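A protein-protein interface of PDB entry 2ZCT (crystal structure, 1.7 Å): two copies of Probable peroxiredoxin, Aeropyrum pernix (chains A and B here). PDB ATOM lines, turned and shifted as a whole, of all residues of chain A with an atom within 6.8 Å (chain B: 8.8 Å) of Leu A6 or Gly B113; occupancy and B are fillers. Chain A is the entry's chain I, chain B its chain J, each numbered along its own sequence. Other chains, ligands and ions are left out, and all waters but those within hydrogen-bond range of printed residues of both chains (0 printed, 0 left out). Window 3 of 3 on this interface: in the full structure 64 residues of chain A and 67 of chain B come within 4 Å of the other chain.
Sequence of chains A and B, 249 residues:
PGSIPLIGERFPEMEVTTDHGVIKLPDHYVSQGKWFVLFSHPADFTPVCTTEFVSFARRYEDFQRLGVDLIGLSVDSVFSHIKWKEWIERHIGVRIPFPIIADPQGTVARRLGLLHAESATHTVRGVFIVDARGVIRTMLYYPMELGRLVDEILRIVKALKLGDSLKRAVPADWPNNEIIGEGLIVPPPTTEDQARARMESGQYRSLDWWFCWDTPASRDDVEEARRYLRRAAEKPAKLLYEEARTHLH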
ATOM      1  N   ILE A   4      18.191 -11.799 -32.005  1.00  0.00           N
ATOM      2  CA  ILE A   4      17.862 -10.558 -32.750  1.00  0.00           C
ATOM      3  C   ILE A   4      16.516 -10.619 -33.458  1.00  0.00           C
ATOM      4  O   ILE A   4      15.957  -9.557 -33.722  1.00  0.00           O
ATOM      5  CB  ILE A   4      18.953 -10.152 -33.784  1.00  0.00           C
ATOM      6  CG1 ILE A   4      19.132 -11.235 -34.862  1.00  0.00           C
ATOM      7  CG2 ILE A   4      20.211  -9.757 -33.058  1.00  0.00           C
ATOM      8  CD1 ILE A   4      20.449 -11.222 -35.601  1.00  0.00           C
ATOM      9  N   PRO A   5      16.013 -11.828 -33.816  1.00  0.00           N
ATOM     10  CA  PRO A   5      14.659 -11.815 -34.381  1.00  0.00           C
ATOM     11  C   PRO A   5      13.709 -11.343 -33.300  1.00  0.00           C
ATOM     12  O   PRO A   5      13.806 -11.835 -32.171  1.00  0.00           O
ATOM     13  CB  PRO A   5      14.393 -13.288 -34.725  1.00  0.00           C
ATOM     14  CG  PRO A   5      15.397 -14.075 -33.974  1.00  0.00           C
ATOM     15  CD  PRO A   5      16.583 -13.196 -33.771  1.00  0.00           C
ATOM     16  N   LEU A   6      12.812 -10.404 -33.636  1.00  0.00           N
ATOM     17  CA  LEU A   6      11.998  -9.703 -32.651  1.00  0.00           C
ATOM     18  C   LEU A   6      10.723 -10.451 -32.320  1.00  0.00           C
ATOM     19  O   LEU A   6      10.257 -11.260 -33.118  1.00  0.00           O
ATOM     20  CB  LEU A   6      11.604  -8.318 -33.183  1.00  0.00           C
ATOM     21  CG  LEU A   6      12.414  -7.061 -32.852  1.00  0.00           C
ATOM     22  CD1 LEU A   6      13.892  -7.291 -32.927  1.00  0.00           C
ATOM     23  CD2 LEU A   6      11.996  -5.938 -33.789  1.00  0.00           C
ATOM     24  N   ILE A   7      10.146 -10.132 -31.161  1.00  0.00           N
ATOM     25  CA  ILE A   7       8.835 -10.650 -30.813  1.00  0.00           C
ATOM     26  C   ILE A   7       7.877 -10.266 -31.923  1.00  0.00           C
ATOM     27  O   ILE A   7       7.948  -9.148 -32.495  1.00  0.00           O
ATOM     28  CB  ILE A   7       8.321 -10.185 -29.410  1.00  0.00           C
ATOM     29  CG1 ILE A   7       8.414  -8.660 -29.257  1.00  0.00           C
ATOM     30  CG2 ILE A   7       9.078 -10.910 -28.273  1.00  0.00           C
ATOM     31  CD1 ILE A   7       8.072  -8.118 -27.826  1.00  0.00           C
ATOM     32  N   GLY A   8       7.016 -11.205 -32.274  1.00  0.00           N
ATOM     33  CA  GLY A   8       6.057 -10.977 -33.326  1.00  0.00           C
ATOM     34  C   GLY A   8       6.552 -11.386 -34.693  1.00  0.00           C
ATOM     35  O   GLY A   8       5.759 -11.501 -35.610  1.00  0.00           O
ATOM     36  N   GLU A   9       7.854 -11.609 -34.831  1.00  0.00           N
ATOM     37  CA  GLU A   9       8.424 -12.086 -36.095  1.00  0.00           C
ATOM     38  C   GLU A   9       8.426 -13.605 -36.140  1.00  0.00           C
ATOM     39  O   GLU A   9       8.455 -14.261 -35.088  1.00  0.00           O
ATOM     40  CB  GLU A   9       9.846 -11.537 -36.308  1.00  0.00           C
ATOM     41  CG  GLU A   9       9.905 -10.000 -36.385  1.00  0.00           C
ATOM     42  CD  GLU A   9      11.341  -9.423 -36.529  1.00  0.00           C
ATOM     43  OE1 GLU A   9      12.334 -10.192 -36.580  1.00  0.00           O
ATOM     44  OE2 GLU A   9      11.466  -8.169 -36.590  1.00  0.00           O
ATOM     45  N   ARG A  10       8.375 -14.160 -37.346  1.00  0.00           N
ATOM     46  CA  ARG A  10       8.440 -15.609 -37.488  1.00  0.00           C
ATOM     47  C   ARG A  10       9.827 -16.095 -37.050  1.00  0.00           C
ATOM     48  O   ARG A  10      10.852 -15.428 -37.278  1.00  0.00           O
ATOM     49  CB  ARG A  10       8.108 -16.048 -38.916  1.00  0.00           C
ATOM     50  CG  ARG A  10       7.900 -17.561 -39.028  1.00  0.00           C
ATOM     51  CD  ARG A  10       7.342 -18.015 -40.369  1.00  0.00           C
ATOM     52  NE  ARG A  10       6.544 -19.225 -40.173  1.00  0.00           N
ATOM     53  CZ  ARG A  10       6.936 -20.467 -40.455  1.00  0.00           C
ATOM     54  NH1 ARG A  10       8.138 -20.715 -40.969  1.00  0.00           N
ATOM     55  NH2 ARG A  10       6.105 -21.478 -40.217  1.00  0.00           N
ATOM     56  N   PHE A 128      13.738 -18.489 -26.530  1.00  0.00           N
ATOM     57  CA  PHE A 128      12.720 -18.057 -27.485  1.00  0.00           C
ATOM     58  C   PHE A 128      11.482 -18.902 -27.248  1.00  0.00           C
ATOM     59  O   PHE A 128      11.582 -20.121 -27.261  1.00  0.00           O
ATOM     60  CB  PHE A 128      13.218 -18.255 -28.930  1.00  0.00           C
ATOM     61  CG  PHE A 128      14.446 -17.435 -29.237  1.00  0.00           C
ATOM     62  CD1 PHE A 128      15.710 -17.929 -28.955  1.00  0.00           C
ATOM     63  CD2 PHE A 128      14.317 -16.146 -29.759  1.00  0.00           C
ATOM     64  CE1 PHE A 128      16.846 -17.160 -29.219  1.00  0.00           C
ATOM     65  CE2 PHE A 128      15.444 -15.380 -30.037  1.00  0.00           C
ATOM     66  CZ  PHE A 128      16.702 -15.889 -29.749  1.00  0.00           C
ATOM     67  N   VAL A 135       5.588 -18.093 -34.686  1.00  0.00           N
ATOM     68  CA  VAL A 135       5.870 -16.700 -34.358  1.00  0.00           C
ATOM     69  C   VAL A 135       6.510 -16.601 -32.969  1.00  0.00           C
ATOM     70  O   VAL A 135       6.000 -17.164 -31.994  1.00  0.00           O
ATOM     71  CB  VAL A 135       4.556 -15.840 -34.410  1.00  0.00           C
ATOM     72  CG1 VAL A 135       4.800 -14.428 -33.886  1.00  0.00           C
ATOM     73  CG2 VAL A 135       3.978 -15.792 -35.825  1.00  0.00           C
ATOM     74  N   ILE A 136       7.636 -15.890 -32.880  1.00  0.00           N
ATOM     75  CA  ILE A 136       8.274 -15.613 -31.590  1.00  0.00           C
ATOM     76  C   ILE A 136       7.377 -14.706 -30.731  1.00  0.00           C
ATOM     77  O   ILE A 136       7.014 -13.596 -31.142  1.00  0.00           O
ATOM     78  CB  ILE A 136       9.652 -14.939 -31.794  1.00  0.00           C
ATOM     79  CG1 ILE A 136      10.563 -15.862 -32.600  1.00  0.00           C
ATOM     80  CG2 ILE A 136      10.305 -14.537 -30.437  1.00  0.00           C
ATOM     81  CD1 ILE A 136      11.823 -15.185 -33.070  1.00  0.00           C
ATOM     82  N   ARG A 137       7.021 -15.198 -29.544  1.00  0.00           N
ATOM     83  CA  ARG A 137       6.061 -14.508 -28.671  1.00  0.00           C
ATOM     84  C   ARG A 137       6.703 -13.837 -27.451  1.00  0.00           C
ATOM     85  O   ARG A 137       6.153 -12.859 -26.942  1.00  0.00           O
ATOM     86  CB  ARG A 137       4.980 -15.488 -28.198  1.00  0.00           C
ATOM     87  CG  ARG A 137       4.152 -16.140 -29.369  1.00  0.00           C
ATOM     88  CD  ARG A 137       3.424 -15.063 -30.207  1.00  0.00           C
ATOM     89  NE  ARG A 137       2.484 -14.357 -29.334  1.00  0.00           N
ATOM     90  CZ  ARG A 137       1.274 -14.804 -28.977  1.00  0.00           C
ATOM     91  NH1 ARG A 137       0.797 -15.943 -29.482  1.00  0.00           N
ATOM     92  NH2 ARG A 137       0.513 -14.099 -28.144  1.00  0.00           N
ATOM     93  N   MET A 139      10.962 -13.442 -25.444  1.00  0.00           N
ATOM     94  CA  MET A 139      12.370 -13.827 -25.464  1.00  0.00           C
ATOM     95  C   MET A 139      12.982 -13.435 -24.124  1.00  0.00           C
ATOM     96  O   MET A 139      12.709 -12.337 -23.626  1.00  0.00           O
ATOM     97  CB  MET A 139      13.071 -13.219 -26.705  1.00  0.00           C
ATOM     98  CG  MET A 139      14.314 -12.338 -26.550  1.00  0.00           C
ATOM     99  SD  MET A 139      15.855 -12.985 -25.888  1.00  0.00           S
ATOM    100  CE  MET A 139      17.112 -12.590 -27.135  1.00  0.00           C
ATOM    101  N   ILE B   4      19.135  -5.855 -29.418  1.00  0.00           N
ATOM    102  CA  ILE B   4      20.406  -5.928 -30.205  1.00  0.00           C
ATOM    103  C   ILE B   4      21.716  -5.784 -29.388  1.00  0.00           C
ATOM    104  O   ILE B   4      22.684  -6.471 -29.703  1.00  0.00           O
ATOM    105  CB  ILE B   4      20.409  -5.068 -31.542  1.00  0.00           C
ATOM    106  CG1 ILE B   4      20.329  -3.565 -31.295  1.00  0.00           C
ATOM    107  CG2 ILE B   4      19.291  -5.500 -32.502  1.00  0.00           C
ATOM    108  CD1 ILE B   4      21.626  -2.853 -31.422  1.00  0.00           C
ATOM    109  N   PRO B   5      21.767  -4.896 -28.355  1.00  0.00           N
ATOM    110  CA  PRO B   5      22.982  -4.972 -27.536  1.00  0.00           C
ATOM    111  C   PRO B   5      22.933  -6.164 -26.582  1.00  0.00           C
ATOM    112  O   PRO B   5      21.943  -6.327 -25.874  1.00  0.00           O
ATOM    113  CB  PRO B   5      22.987  -3.643 -26.766  1.00  0.00           C
ATOM    114  CG  PRO B   5      21.569  -3.204 -26.728  1.00  0.00           C
ATOM    115  CD  PRO B   5      20.847  -3.836 -27.882  1.00  0.00           C
ATOM    116  N   PRO B  12      24.496   1.109 -24.341  1.00  0.00           N
ATOM    117  CA  PRO B  12      24.822   2.141 -25.333  1.00  0.00           C
ATOM    118  C   PRO B  12      24.776   3.560 -24.758  1.00  0.00           C
ATOM    119  O   PRO B  12      23.804   3.959 -24.091  1.00  0.00           O
ATOM    120  CB  PRO B  12      23.732   1.971 -26.386  1.00  0.00           C
ATOM    121  CG  PRO B  12      23.330   0.543 -26.290  1.00  0.00           C
ATOM    122  CD  PRO B  12      23.495   0.160 -24.845  1.00  0.00           C
ATOM    123  N   MET B  14      24.191   7.346 -24.493  1.00  0.00           N
ATOM    124  CA  MET B  14      23.146   8.184 -25.076  1.00  0.00           C
ATOM    125  C   MET B  14      22.686   9.264 -24.131  1.00  0.00           C
ATOM    126  O   MET B  14      22.649   9.074 -22.914  1.00  0.00           O
ATOM    127  CB  MET B  14      21.930   7.333 -25.457  1.00  0.00           C
ATOM    128  CG  MET B  14      21.386   6.507 -24.297  1.00  0.00           C
ATOM    129  SD  MET B  14      19.928   5.549 -24.802  1.00  0.00           S
ATOM    130  CE  MET B  14      20.692   4.210 -25.714  1.00  0.00           C
ATOM    131  N   LEU B  73      10.576   3.718 -20.288  1.00  0.00           N
ATOM    132  CA  LEU B  73      10.769   4.298 -21.622  1.00  0.00           C
ATOM    133  C   LEU B  73       9.452   4.072 -22.355  1.00  0.00           C
ATOM    134  O   LEU B  73       8.917   2.985 -22.281  1.00  0.00           O
ATOM    135  CB  LEU B  73      11.885   3.605 -22.400  1.00  0.00           C
ATOM    136  CG  LEU B  73      12.093   3.794 -23.919  1.00  0.00           C
ATOM    137  CD1 LEU B  73      12.583   5.200 -24.215  1.00  0.00           C
ATOM    138  CD2 LEU B  73      13.115   2.774 -24.446  1.00  0.00           C
ATOM    139  N   GLY B 106      10.981   7.691 -31.473  1.00  0.00           N
ATOM    140  CA  GLY B 106      11.524   6.349 -31.232  1.00  0.00           C
ATOM    141  C   GLY B 106      13.028   6.163 -31.369  1.00  0.00           C
ATOM    142  O   GLY B 106      13.507   5.048 -31.558  1.00  0.00           O
ATOM    143  N   THR B 107      13.770   7.259 -31.245  1.00  0.00           N
ATOM    144  CA  THR B 107      15.228   7.259 -31.368  1.00  0.00           C
ATOM    145  C   THR B 107      15.938   6.295 -30.410  1.00  0.00           C
ATOM    146  O   THR B 107      16.794   5.497 -30.818  1.00  0.00           O
ATOM    147  CB  THR B 107      15.728   8.668 -31.144  1.00  0.00           C
ATOM    148  OG1 THR B 107      15.101   9.530 -32.114  1.00  0.00           O
ATOM    149  CG2 THR B 107      17.249   8.747 -31.256  1.00  0.00           C
ATOM    150  N   VAL B 108      15.597   6.412 -29.133  1.00  0.00           N
ATOM    151  CA  VAL B 108      16.134   5.540 -28.102  1.00  0.00           C
ATOM    152  C   VAL B 108      15.730   4.081 -28.322  1.00  0.00           C
ATOM    153  O   VAL B 108      16.580   3.178 -28.237  1.00  0.00           O
ATOM    154  CB  VAL B 108      15.685   5.978 -26.706  1.00  0.00           C
ATOM    155  CG1 VAL B 108      16.250   5.012 -25.650  1.00  0.00           C
ATOM    156  CG2 VAL B 108      16.092   7.432 -26.428  1.00  0.00           C
ATOM    157  N   ALA B 109      14.449   3.846 -28.629  1.00  0.00           N
ATOM    158  CA  ALA B 109      13.954   2.486 -28.885  1.00  0.00           C
ATOM    159  C   ALA B 109      14.698   1.841 -30.058  1.00  0.00           C
ATOM    160  O   ALA B 109      15.073   0.683 -29.995  1.00  0.00           O
ATOM    161  CB  ALA B 109      12.437   2.507 -29.127  1.00  0.00           C
ATOM    162  N   ARG B 110      14.979   2.616 -31.105  1.00  0.00           N
ATOM    163  CA  ARG B 110      15.711   2.085 -32.262  1.00  0.00           C
ATOM    164  C   ARG B 110      17.168   1.798 -31.940  1.00  0.00           C
ATOM    165  O   ARG B 110      17.740   0.838 -32.457  1.00  0.00           O
ATOM    166  CB  ARG B 110      15.665   3.074 -33.422  1.00  0.00           C
ATOM    167  CG  ARG B 110      14.314   3.164 -34.065  1.00  0.00           C
ATOM    168  CD  ARG B 110      14.388   3.845 -35.426  1.00  0.00           C
ATOM    169  NE  ARG B 110      13.136   4.544 -35.633  1.00  0.00           N
ATOM    170  CZ  ARG B 110      12.948   5.847 -35.431  1.00  0.00           C
ATOM    171  NH1 ARG B 110      13.957   6.645 -35.063  1.00  0.00           N
ATOM    172  NH2 ARG B 110      11.740   6.362 -35.635  1.00  0.00           N
ATOM    173  N   ARG B 111      17.766   2.650 -31.108  1.00  0.00           N
ATOM    174  CA  ARG B 111      19.159   2.505 -30.702  1.00  0.00           C
ATOM    175  C   ARG B 111      19.350   1.226 -29.882  1.00  0.00           C
ATOM    176  O   ARG B 111      20.391   0.576 -29.957  1.00  0.00           O
ATOM    177  CB  ARG B 111      19.616   3.729 -29.900  1.00  0.00           C
ATOM    178  CG  ARG B 111      21.073   4.119 -30.183  1.00  0.00           C
ATOM    179  CD  ARG B 111      22.047   3.499 -29.208  1.00  0.00           C
ATOM    180  NE  ARG B 111      23.400   3.313 -29.761  1.00  0.00           N
ATOM    181  CZ  ARG B 111      23.926   2.120 -30.064  1.00  0.00           C
ATOM    182  NH1 ARG B 111      23.229   1.000 -29.879  1.00  0.00           N
ATOM    183  NH2 ARG B 111      25.163   2.036 -30.541  1.00  0.00           N
ATOM    184  N   LEU B 112      18.317   0.861 -29.122  1.00  0.00           N
ATOM    185  CA  LEU B 112      18.307  -0.341 -28.287  1.00  0.00           C
ATOM    186  C   LEU B 112      17.802  -1.578 -29.042  1.00  0.00           C
ATOM    187  O   LEU B 112      17.633  -2.651 -28.457  1.00  0.00           O
ATOM    188  CB  LEU B 112      17.432  -0.094 -27.054  1.00  0.00           C
ATOM    189  CG  LEU B 112      18.023   0.937 -26.096  1.00  0.00           C
ATOM    190  CD1 LEU B 112      17.069   1.195 -24.944  1.00  0.00           C
ATOM    191  CD2 LEU B 112      19.385   0.470 -25.562  1.00  0.00           C
ATOM    192  N   GLY B 113      17.560  -1.421 -30.332  1.00  0.00           N
ATOM    193  CA  GLY B 113      17.174  -2.537 -31.187  1.00  0.00           C
ATOM    194  C   GLY B 113      15.746  -2.995 -30.976  1.00  0.00           C
ATOM    195  O   GLY B 113      15.387  -4.109 -31.399  1.00  0.00           O
ATOM    196  N   LEU B 114      14.932  -2.135 -30.360  1.00  0.00           N
ATOM    197  CA  LEU B 114      13.534  -2.442 -30.022  1.00  0.00           C
ATOM    198  C   LEU B 114      12.505  -2.161 -31.125  1.00  0.00           C
ATOM    199  O   LEU B 114      11.346  -2.519 -30.993  1.00  0.00           O
ATOM    200  CB  LEU B 114      13.112  -1.674 -28.763  1.00  0.00           C
ATOM    201  CG  LEU B 114      13.784  -2.028 -27.434  1.00  0.00           C
ATOM    202  CD1 LEU B 114      13.359  -1.095 -26.327  1.00  0.00           C
ATOM    203  CD2 LEU B 114      13.501  -3.464 -27.019  1.00  0.00           C
ATOM    204  N   LEU B 115      12.938  -1.493 -32.186  1.00  0.00           N
ATOM    205  CA  LEU B 115      12.036  -0.915 -33.163  1.00  0.00           C
ATOM    206  C   LEU B 115      12.663  -1.074 -34.531  1.00  0.00           C
ATOM    207  O   LEU B 115      13.749  -0.516 -34.742  1.00  0.00           O
ATOM    208  CB  LEU B 115      11.905   0.584 -32.882  1.00  0.00           C
ATOM    209  CG  LEU B 115      10.571   1.237 -32.575  1.00  0.00           C
ATOM    210  CD1 LEU B 115      10.728   2.729 -32.733  1.00  0.00           C
ATOM    211  CD2 LEU B 115       9.442   0.698 -33.450  1.00  0.00           C
ATOM    212  N   ALA B 120       4.952  -0.126 -36.401  1.00  0.00           N
ATOM    213  CA  ALA B 120       4.148   0.220 -35.215  1.00  0.00           C
ATOM    214  C   ALA B 120       5.112   0.101 -34.034  1.00  0.00           C
ATOM    215  O   ALA B 120       6.251  -0.288 -34.238  1.00  0.00           O
ATOM    216  CB  ALA B 120       2.963  -0.721 -35.077  1.00  0.00           C
ATOM    217  N   HIS B 122       4.661  -1.773 -31.150  1.00  0.00           N
ATOM    218  CA  HIS B 122       4.352  -2.939 -30.284  1.00  0.00           C
ATOM    219  C   HIS B 122       5.557  -3.676 -29.732  1.00  0.00           C
ATOM    220  O   HIS B 122       5.453  -4.355 -28.704  1.00  0.00           O
ATOM    221  CB  HIS B 122       3.497  -3.994 -31.032  1.00  0.00           C
ATOM    222  CG  HIS B 122       2.333  -3.419 -31.784  1.00  0.00           C
ATOM    223  ND1 HIS B 122       1.411  -2.573 -31.202  1.00  0.00           N
ATOM    224  CD2 HIS B 122       1.935  -3.584 -33.068  1.00  0.00           C
ATOM    225  CE1 HIS B 122       0.496  -2.237 -32.099  1.00  0.00           C
ATOM    226  NE2 HIS B 122       0.797  -2.831 -33.240  1.00  0.00           N
ATOM    227  N   THR B 123       6.681  -3.620 -30.453  1.00  0.00           N
ATOM    228  CA  THR B 123       7.883  -4.326 -30.045  1.00  0.00           C
ATOM    229  C   THR B 123       8.701  -3.556 -29.008  1.00  0.00           C
ATOM    230  O   THR B 123       9.707  -4.080 -28.512  1.00  0.00           O
ATOM    231  CB  THR B 123       8.811  -4.647 -31.254  1.00  0.00           C
ATOM    232  OG1 THR B 123       9.102  -3.438 -31.989  1.00  0.00           O
ATOM    233  CG2 THR B 123       8.156  -5.716 -32.168  1.00  0.00           C
ATOM    234  N   VAL B 124       8.274  -2.329 -28.674  1.00  0.00           N
ATOM    235  CA  VAL B 124       8.998  -1.501 -27.659  1.00  0.00           C
ATOM    236  C   VAL B 124       8.639  -1.983 -26.255  1.00  0.00           C
ATOM    237  O   VAL B 124       7.796  -1.408 -25.542  1.00  0.00           O
ATOM    238  CB  VAL B 124       8.775   0.012 -27.873  1.00  0.00           C
ATOM    239  CG1 VAL B 124       9.584   0.859 -26.866  1.00  0.00           C
ATOM    240  CG2 VAL B 124       9.162   0.388 -29.343  1.00  0.00           C
ATOM    241  N   ARG B 125       9.279  -3.076 -25.875  1.00  0.00           N
ATOM    242  CA  ARG B 125       8.906  -3.843 -24.669  1.00  0.00           C
ATOM    243  C   ARG B 125      10.107  -4.395 -23.888  1.00  0.00           C
ATOM    244  O   ARG B 125       9.940  -5.123 -22.896  1.00  0.00           O
ATOM    245  CB  ARG B 125       8.018  -5.013 -25.080  1.00  0.00           C
ATOM    246  CG  ARG B 125       6.624  -4.582 -25.391  1.00  0.00           C
ATOM    247  CD  ARG B 125       5.933  -4.096 -24.106  1.00  0.00           C
ATOM    248  NE  ARG B 125       5.675  -5.225 -23.199  1.00  0.00           N
ATOM    249  CZ  ARG B 125       5.302  -5.088 -21.939  1.00  0.00           C
ATOM    250  NH1 ARG B 125       5.201  -3.862 -21.427  1.00  0.00           N
ATOM    251  NH2 ARG B 125       5.035  -6.162 -21.182  1.00  0.00           N
ATOM    252  N   GLY B 126      11.313  -4.081 -24.341  1.00  0.00           N
ATOM    253  CA  GLY B 126      12.492  -4.601 -23.670  1.00  0.00           C
ATOM    254  C   GLY B 126      12.669  -4.139 -22.239  1.00  0.00           C
ATOM    255  O   GLY B 126      12.376  -2.976 -21.898  1.00  0.00           O
ATOM    256  N   PHE B 128      15.956  -3.998 -19.616  1.00  0.00           N
ATOM    257  CA  PHE B 128      17.420  -4.089 -19.552  1.00  0.00           C
ATOM    258  C   PHE B 128      17.825  -3.915 -18.112  1.00  0.00           C
ATOM    259  O   PHE B 128      17.492  -2.911 -17.506  1.00  0.00           O
ATOM    260  CB  PHE B 128      18.081  -2.995 -20.402  1.00  0.00           C
ATOM    261  CG  PHE B 128      17.682  -3.035 -21.860  1.00  0.00           C
ATOM    262  CD1 PHE B 128      16.473  -2.474 -22.269  1.00  0.00           C
ATOM    263  CD2 PHE B 128      18.493  -3.674 -22.801  1.00  0.00           C
ATOM    264  CE1 PHE B 128      16.084  -2.513 -23.589  1.00  0.00           C
ATOM    265  CE2 PHE B 128      18.126  -3.719 -24.139  1.00  0.00           C
ATOM    266  CZ  PHE B 128      16.915  -3.134 -24.534  1.00  0.00           C
ATOM    267  N   MET B 139      18.382  -9.325 -20.076  1.00  0.00           N
ATOM    268  CA  MET B 139      17.383  -8.628 -20.877  1.00  0.00           C
ATOM    269  C   MET B 139      16.150  -9.530 -20.917  1.00  0.00           C
ATOM    270  O   MET B 139      16.279 -10.759 -21.021  1.00  0.00           O
ATOM    271  CB  MET B 139      17.898  -8.319 -22.278  1.00  0.00           C
ATOM    272  CG  MET B 139      18.969  -7.234 -22.276  1.00  0.00           C
ATOM    273  SD  MET B 139      19.623  -6.879 -23.919  1.00  0.00           S
ATOM    274  CE  MET B 139      20.725  -8.263 -24.150  1.00  0.00           C
ATOM    275  N   TYR B 141      12.169  -9.762 -22.685  1.00  0.00           N
ATOM    276  CA  TYR B 141      11.282  -9.265 -23.730  1.00  0.00           C
ATOM    277  C   TYR B 141       9.916  -9.952 -23.647  1.00  0.00           C
ATOM    278  O   TYR B 141       9.619 -10.903 -24.378  1.00  0.00           O
ATOM    279  CB  TYR B 141      11.881  -9.436 -25.117  1.00  0.00           C
ATOM    280  CG  TYR B 141      13.156  -8.688 -25.327  1.00  0.00           C
ATOM    281  CD1 TYR B 141      14.394  -9.266 -25.005  1.00  0.00           C
ATOM    282  CD2 TYR B 141      13.140  -7.388 -25.856  1.00  0.00           C
ATOM    283  CE1 TYR B 141      15.585  -8.561 -25.189  1.00  0.00           C
ATOM    284  CE2 TYR B 141      14.323  -6.685 -26.050  1.00  0.00           C
ATOM    285  CZ  TYR B 141      15.529  -7.271 -25.714  1.00  0.00           C
ATOM    286  OH  TYR B 141      16.681  -6.578 -25.926  1.00  0.00           O
ATOM    287  N   PRO B 143       5.975  -9.527 -24.377  1.00  0.00           N
ATOM    288  CA  PRO B 143       5.305  -8.774 -25.410  1.00  0.00           C
ATOM    289  C   PRO B 143       4.253  -7.834 -24.816  1.00  0.00           C
ATOM    290  O   PRO B 143       3.935  -7.936 -23.628  1.00  0.00           O
ATOM    291  CB  PRO B 143       4.645  -9.872 -26.269  1.00  0.00           C
ATOM    292  CG  PRO B 143       4.314 -10.938 -25.313  1.00  0.00           C
ATOM    293  CD  PRO B 143       5.442 -10.908 -24.267  1.00  0.00           C
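The backbone carbonyl oxygen (O) of Met A139 sits at hydrogen-bond distance from the backbone NH (N) of Tyr B141, 2.8 Å away.
The backbone carbonyl oxygen (O) of Pro B143 sits at hydrogen-bond distance from the guanidinium group (NH2) of Arg B125, 3.2 Å away.
N of Leu A6 lies within hydrogen-bond range of OE1 of Glu A9 (3.0 Å).
OH of Tyr B141 sits at hydrogen-bond distance from SD of Met B139 (3.6 Å).
The side-chain hydroxyl (OG1) of Thr B123 is in hydrogen-bond range of the backbone carbonyl oxygen (O) of Leu B114, at 2.6 Å.
Gly B113 touches Leu A6.
Thr B123 touches Ile A7.
Ile A7 touches Tyr B141 (CG2 to O, 3.9 Å).
CD1 of Ile A7 touches CA of Pro B143, at 3.7 Å.
Pro B143 touches Arg A137 (CG to O, 3.1 Å).
No residue of chain B comes within 4 Å of Pro A5.
Of chain B, only Gly B113 (3.8 Å) comes within 4 Å of Leu A6.
Of the printed residues of chain B, Ile A7 touches Thr B123, Tyr B141 and Pro B143.
Glu A9 touches none of the printed residues of chain B.
Of the printed residues of chain B, Arg A137 touches Pro B143 (3.1 Å).
Printed residues of chain B within 4 Å of Met A139: Tyr B141 (2.8 Å).
Gly B113 touches just one residue of chain A: Leu A6 (3.8 Å).
Printed residues of chain A within 4 Å of Tyr B141: Ile A7 and Met A139.
Of the printed residues of chain A, Pro B143 touches Ile A7 and Arg A137.
The nearest residue of chain B that does not touch Leu A6 is Thr B123 (4.2 Å).
Of the 12 printed residues of chain A, 4 touch a printed residue of chain B.
Printed residues of chain B that touch a printed residue of chain A: Gly B113, Thr B123, Tyr B141 and Pro B143.
Among the printed residues, no Asp or Glu carboxylate lies within 4 Å of a Lys or Arg side-chain nitrogen of the other chain.
Positions printed for both chains: 4, 5, 128 and 139.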
